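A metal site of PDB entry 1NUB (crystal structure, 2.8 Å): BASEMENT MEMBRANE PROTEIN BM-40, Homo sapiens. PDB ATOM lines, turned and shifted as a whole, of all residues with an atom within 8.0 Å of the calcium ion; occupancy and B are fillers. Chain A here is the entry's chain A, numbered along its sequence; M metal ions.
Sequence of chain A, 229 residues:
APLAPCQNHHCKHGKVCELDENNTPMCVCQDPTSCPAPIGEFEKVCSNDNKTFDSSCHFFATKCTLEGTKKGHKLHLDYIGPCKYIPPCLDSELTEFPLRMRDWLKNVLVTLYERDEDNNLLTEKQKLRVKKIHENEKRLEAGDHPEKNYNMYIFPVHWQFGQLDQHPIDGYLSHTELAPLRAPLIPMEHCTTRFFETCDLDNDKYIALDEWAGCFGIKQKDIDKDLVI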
ATOM      1  N   TYR A 172      12.108  14.567 -17.973  1.00  0.00           N
ATOM      2  CA  TYR A 172      12.360  13.687 -19.116  1.00  0.00           C
ATOM      3  C   TYR A 172      11.320  12.582 -19.094  1.00  0.00           C
ATOM      4  O   TYR A 172      10.781  12.250 -18.051  1.00  0.00           O
ATOM      5  CB  TYR A 172      13.749  13.056 -19.004  1.00  0.00           C
ATOM      6  CG  TYR A 172      14.878  14.030 -18.823  1.00  0.00           C
ATOM      7  CD1 TYR A 172      15.270  14.440 -17.558  1.00  0.00           C
ATOM      8  CD2 TYR A 172      15.552  14.553 -19.931  1.00  0.00           C
ATOM      9  CE1 TYR A 172      16.304  15.348 -17.375  1.00  0.00           C
ATOM     10  CE2 TYR A 172      16.585  15.467 -19.755  1.00  0.00           C
ATOM     11  CZ  TYR A 172      16.956  15.865 -18.483  1.00  0.00           C
ATOM     12  OH  TYR A 172      17.973  16.769 -18.313  1.00  0.00           O
ATOM     13  N   LEU A 173      11.026  12.032 -20.258  1.00  0.00           N
ATOM     14  CA  LEU A 173      10.061  10.942 -20.328  1.00  0.00           C
ATOM     15  C   LEU A 173      10.803   9.677 -20.755  1.00  0.00           C
ATOM     16  O   LEU A 173      11.540   9.676 -21.754  1.00  0.00           O
ATOM     17  CB  LEU A 173       8.942  11.250 -21.328  1.00  0.00           C
ATOM     18  CG  LEU A 173       8.138  12.528 -21.101  1.00  0.00           C
ATOM     19  CD1 LEU A 173       7.088  12.666 -22.175  1.00  0.00           C
ATOM     20  CD2 LEU A 173       7.510  12.488 -19.738  1.00  0.00           C
ATOM     21  N   PHE A 196       8.925   8.678 -31.040  1.00  0.00           N
ATOM     22  CA  PHE A 196       9.706   9.254 -29.972  1.00  0.00           C
ATOM     23  C   PHE A 196      11.190   8.967 -30.065  1.00  0.00           C
ATOM     24  O   PHE A 196      11.991   9.826 -29.710  1.00  0.00           O
ATOM     25  CB  PHE A 196       9.081   8.964 -28.605  1.00  0.00           C
ATOM     26  CG  PHE A 196       7.834   9.762 -28.348  1.00  0.00           C
ATOM     27  CD1 PHE A 196       7.905  11.130 -28.119  1.00  0.00           C
ATOM     28  CD2 PHE A 196       6.588   9.147 -28.395  1.00  0.00           C
ATOM     29  CE1 PHE A 196       6.761  11.883 -27.956  1.00  0.00           C
ATOM     30  CE2 PHE A 196       5.430   9.901 -28.229  1.00  0.00           C
ATOM     31  CZ  PHE A 196       5.507  11.263 -28.006  1.00  0.00           C
ATOM     32  N   GLU A 197      11.551   7.801 -30.602  1.00  0.00           N
ATOM     33  CA  GLU A 197      12.965   7.480 -30.788  1.00  0.00           C
ATOM     34  C   GLU A 197      13.463   8.588 -31.712  1.00  0.00           C
ATOM     35  O   GLU A 197      14.461   9.237 -31.433  1.00  0.00           O
ATOM     36  CB  GLU A 197      13.134   6.100 -31.437  1.00  0.00           C
ATOM     37  CG  GLU A 197      12.910   4.886 -30.508  1.00  0.00           C
ATOM     38  CD  GLU A 197      12.741   3.556 -31.262  1.00  0.00           C
ATOM     39  OE1 GLU A 197      12.671   3.576 -32.510  1.00  0.00           O
ATOM     40  OE2 GLU A 197      12.675   2.497 -30.601  1.00  0.00           O
ATOM     41  N   CYS A 199      12.541  11.407 -31.886  1.00  0.00           N
ATOM     42  CA  CYS A 199      12.636  12.639 -31.095  1.00  0.00           C
ATOM     43  C   CYS A 199      13.830  12.695 -30.150  1.00  0.00           C
ATOM     44  O   CYS A 199      14.275  13.778 -29.792  1.00  0.00           O
ATOM     45  CB  CYS A 199      11.351  12.845 -30.295  1.00  0.00           C
ATOM     46  SG  CYS A 199       9.824  12.702 -31.275  1.00  0.00           S
ATOM     47  N   ASP A 200      14.325  11.523 -29.738  1.00  0.00           N
ATOM     48  CA  ASP A 200      15.468  11.403 -28.810  1.00  0.00           C
ATOM     49  C   ASP A 200      16.760  11.888 -29.464  1.00  0.00           C
ATOM     50  O   ASP A 200      17.629  11.095 -29.804  1.00  0.00           O
ATOM     51  CB  ASP A 200      15.606   9.935 -28.391  1.00  0.00           C
ATOM     52  CG  ASP A 200      16.643   9.716 -27.302  1.00  0.00           C
ATOM     53  OD1 ASP A 200      17.109  10.704 -26.688  1.00  0.00           O
ATOM     54  OD2 ASP A 200      16.989   8.535 -27.052  1.00  0.00           O
ATOM     55  N   LEU A 201      16.879  13.195 -29.632  1.00  0.00           N
ATOM     56  CA  LEU A 201      18.040  13.804 -30.265  1.00  0.00           C
ATOM     57  C   LEU A 201      19.394  13.332 -29.768  1.00  0.00           C
ATOM     58  O   LEU A 201      20.131  12.681 -30.527  1.00  0.00           O
ATOM     59  CB  LEU A 201      17.956  15.325 -30.208  1.00  0.00           C
ATOM     60  CG  LEU A 201      16.722  15.881 -30.907  1.00  0.00           C
ATOM     61  CD1 LEU A 201      16.857  17.375 -31.016  1.00  0.00           C
ATOM     62  CD2 LEU A 201      16.592  15.262 -32.287  1.00  0.00           C
ATOM     63  N   ASP A 202      19.743  13.627 -28.522  1.00  0.00           N
ATOM     64  CA  ASP A 202      21.047  13.213 -27.996  1.00  0.00           C
ATOM     65  C   ASP A 202      21.177  11.718 -27.714  1.00  0.00           C
ATOM     66  O   ASP A 202      22.236  11.230 -27.318  1.00  0.00           O
ATOM     67  CB  ASP A 202      21.477  14.064 -26.794  1.00  0.00           C
ATOM     68  CG  ASP A 202      20.470  14.036 -25.664  1.00  0.00           C
ATOM     69  OD1 ASP A 202      19.723  13.051 -25.559  1.00  0.00           O
ATOM     70  OD2 ASP A 202      20.459  15.016 -24.876  1.00  0.00           O
ATOM     71  N   ASN A 203      20.094  10.999 -27.942  1.00  0.00           N
ATOM     72  CA  ASN A 203      20.059   9.567 -27.774  1.00  0.00           C
ATOM     73  C   ASN A 203      20.404   9.062 -26.372  1.00  0.00           C
ATOM     74  O   ASN A 203      21.168   8.099 -26.218  1.00  0.00           O
ATOM     75  CB  ASN A 203      20.961   8.905 -28.821  1.00  0.00           C
ATOM     76  CG  ASN A 203      20.443   7.551 -29.268  1.00  0.00           C
ATOM     77  OD1 ASN A 203      19.692   7.448 -30.230  1.00  0.00           O
ATOM     78  ND2 ASN A 203      20.880   6.499 -28.579  1.00  0.00           N
ATOM     79  N   ASP A 204      19.813   9.670 -25.349  1.00  0.00           N
ATOM     80  CA  ASP A 204      20.037   9.266 -23.946  1.00  0.00           C
ATOM     81  C   ASP A 204      18.869   8.400 -23.470  1.00  0.00           C
ATOM     82  O   ASP A 204      18.827   7.967 -22.316  1.00  0.00           O
ATOM     83  CB  ASP A 204      20.200  10.477 -23.028  1.00  0.00           C
ATOM     84  CG  ASP A 204      18.925  11.264 -22.878  1.00  0.00           C
ATOM     85  OD1 ASP A 204      18.016  11.124 -23.723  1.00  0.00           O
ATOM     86  OD2 ASP A 204      18.827  12.021 -21.890  1.00  0.00           O
ATOM     87  N   LYS A 205      17.926   8.155 -24.369  1.00  0.00           N
ATOM     88  CA  LYS A 205      16.751   7.348 -24.117  1.00  0.00           C
ATOM     89  C   LYS A 205      15.692   8.055 -23.277  1.00  0.00           C
ATOM     90  O   LYS A 205      14.812   7.424 -22.715  1.00  0.00           O
ATOM     91  CB  LYS A 205      17.128   6.005 -23.483  1.00  0.00           C
ATOM     92  CG  LYS A 205      18.105   5.177 -24.289  1.00  0.00           C
ATOM     93  CD  LYS A 205      17.701   5.057 -25.746  1.00  0.00           C
ATOM     94  CE  LYS A 205      18.537   4.007 -26.446  1.00  0.00           C
ATOM     95  NZ  LYS A 205      19.977   4.069 -26.037  1.00  0.00           N
ATOM     96  N   TYR A 206      15.784   9.374 -23.222  1.00  0.00           N
ATOM     97  CA  TYR A 206      14.820  10.189 -22.495  1.00  0.00           C
ATOM     98  C   TYR A 206      14.411  11.322 -23.411  1.00  0.00           C
ATOM     99  O   TYR A 206      15.219  11.833 -24.175  1.00  0.00           O
ATOM    100  CB  TYR A 206      15.458  10.782 -21.243  1.00  0.00           C
ATOM    101  CG  TYR A 206      15.758   9.793 -20.163  1.00  0.00           C
ATOM    102  CD1 TYR A 206      16.963   9.108 -20.138  1.00  0.00           C
ATOM    103  CD2 TYR A 206      14.828   9.521 -19.168  1.00  0.00           C
ATOM    104  CE1 TYR A 206      17.238   8.171 -19.154  1.00  0.00           C
ATOM    105  CE2 TYR A 206      15.083   8.591 -18.175  1.00  0.00           C
ATOM    106  CZ  TYR A 206      16.297   7.924 -18.176  1.00  0.00           C
ATOM    107  OH  TYR A 206      16.557   6.994 -17.197  1.00  0.00           O
ATOM    108  N   ILE A 207      13.131  11.682 -23.387  1.00  0.00           N
ATOM    109  CA  ILE A 207      12.671  12.794 -24.193  1.00  0.00           C
ATOM    110  C   ILE A 207      12.583  14.000 -23.271  1.00  0.00           C
ATOM    111  O   ILE A 207      11.829  13.955 -22.280  1.00  0.00           O
ATOM    112  CB  ILE A 207      11.314  12.528 -24.823  1.00  0.00           C
ATOM    113  CG1 ILE A 207      11.385  11.255 -25.679  1.00  0.00           C
ATOM    114  CG2 ILE A 207      10.869  13.732 -25.635  1.00  0.00           C
ATOM    115  CD1 ILE A 207      12.514  11.250 -26.702  1.00  0.00           C
ATOM    116  N   ALA A 208      13.419  15.001 -23.510  1.00  0.00           N
ATOM    117  CA  ALA A 208      13.416  16.217 -22.700  1.00  0.00           C
ATOM    118  C   ALA A 208      12.359  17.148 -23.269  1.00  0.00           C
ATOM    119  O   ALA A 208      11.924  16.976 -24.410  1.00  0.00           O
ATOM    120  CB  ALA A 208      14.767  16.863 -22.750  1.00  0.00           C
ATOM    121  N   LEU A 209      11.931  18.122 -22.472  1.00  0.00           N
ATOM    122  CA  LEU A 209      10.887  19.051 -22.902  1.00  0.00           C
ATOM    123  C   LEU A 209      11.113  19.671 -24.277  1.00  0.00           C
ATOM    124  O   LEU A 209      10.194  19.708 -25.079  1.00  0.00           O
ATOM    125  CB  LEU A 209      10.647  20.157 -21.864  1.00  0.00           C
ATOM    126  CG  LEU A 209       9.558  21.180 -22.208  1.00  0.00           C
ATOM    127  CD1 LEU A 209       8.245  20.483 -22.506  1.00  0.00           C
ATOM    128  CD2 LEU A 209       9.405  22.149 -21.050  1.00  0.00           C
ATOM    129  N   ASP A 210      12.331  20.141 -24.538  1.00  0.00           N
ATOM    130  CA  ASP A 210      12.627  20.733 -25.845  1.00  0.00           C
ATOM    131  C   ASP A 210      12.556  19.698 -26.963  1.00  0.00           C
ATOM    132  O   ASP A 210      12.122  20.011 -28.074  1.00  0.00           O
ATOM    133  CB  ASP A 210      13.991  21.456 -25.835  1.00  0.00           C
ATOM    134  CG  ASP A 210      15.045  20.727 -25.048  1.00  0.00           C
ATOM    135  OD1 ASP A 210      15.735  19.883 -25.631  1.00  0.00           O
ATOM    136  OD2 ASP A 210      15.164  21.008 -23.837  1.00  0.00           O
ATOM    137  N   GLU A 211      12.929  18.460 -26.647  1.00  0.00           N
ATOM    138  CA  GLU A 211      12.866  17.371 -27.615  1.00  0.00           C
ATOM    139  C   GLU A 211      11.404  17.054 -27.901  1.00  0.00           C
ATOM    140  O   GLU A 211      11.000  16.889 -29.069  1.00  0.00           O
ATOM    141  CB  GLU A 211      13.562  16.122 -27.056  1.00  0.00           C
ATOM    142  CG  GLU A 211      15.054  16.299 -26.864  1.00  0.00           C
ATOM    143  CD  GLU A 211      15.732  14.993 -26.530  1.00  0.00           C
ATOM    144  OE1 GLU A 211      15.442  14.444 -25.451  1.00  0.00           O
ATOM    145  OE2 GLU A 211      16.540  14.495 -27.348  1.00  0.00           O
ATOM    146  N   TRP A 212      10.607  16.995 -26.836  1.00  0.00           N
ATOM    147  CA  TRP A 212       9.184  16.718 -26.927  1.00  0.00           C
ATOM    148  C   TRP A 212       8.488  17.818 -27.725  1.00  0.00           C
ATOM    149  O   TRP A 212       7.852  17.541 -28.745  1.00  0.00           O
ATOM    150  CB  TRP A 212       8.581  16.644 -25.506  1.00  0.00           C
ATOM    151  CG  TRP A 212       7.080  16.638 -25.439  1.00  0.00           C
ATOM    152  CD1 TRP A 212       6.253  17.728 -25.452  1.00  0.00           C
ATOM    153  CD2 TRP A 212       6.223  15.496 -25.364  1.00  0.00           C
ATOM    154  NE1 TRP A 212       4.942  17.324 -25.407  1.00  0.00           N
ATOM    155  CE2 TRP A 212       4.894  15.968 -25.344  1.00  0.00           C
ATOM    156  CE3 TRP A 212       6.462  14.115 -25.309  1.00  0.00           C
ATOM    157  CZ2 TRP A 212       3.803  15.100 -25.275  1.00  0.00           C
ATOM    158  CZ3 TRP A 212       5.371  13.264 -25.240  1.00  0.00           C
ATOM    159  CH2 TRP A 212       4.062  13.764 -25.226  1.00  0.00           C
HETATM  160 CA    CA M   1      17.066  12.758 -25.330  1.00  0.00          CA
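The backbone NH of Leu 201 sits close to the side-chain carboxylate of Glu 211, 2.6 Å away. The side-chain carboxylate (OE1) of Glu 211 lies close to the backbone NH (N) of Ala 208 (2.9 Å). OD1 of Asp 200 sits close to N of Asn 203 (3.3 Å). The side-chain carboxylate (OD2) of Asp 200 lies within hydrogen-bond range of the backbone NH (N) of Lys 205 (2.9 Å).
Along chain A the residues within 4 Å of the calcium ion span positions 200 to 211.
The side-chain carboxylate (OE1) of Glu 211 binds the calcium ion (2.3 Å). O of Tyr 206 is bound to the calcium ion, 2.4 Å away. OD1 of Asp 200 binds the calcium ion (2.5 Å). The side-chain carboxylate (OD1) of Asp 204 is bound to the calcium ion, 2.5 Å away. OD1 of Asp 202 is bound to the calcium ion (2.7 Å). The calcium ion is bound by OE2 of Glu 211 (2.7 Å). The calcium ion has six donor atoms within binding distance.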
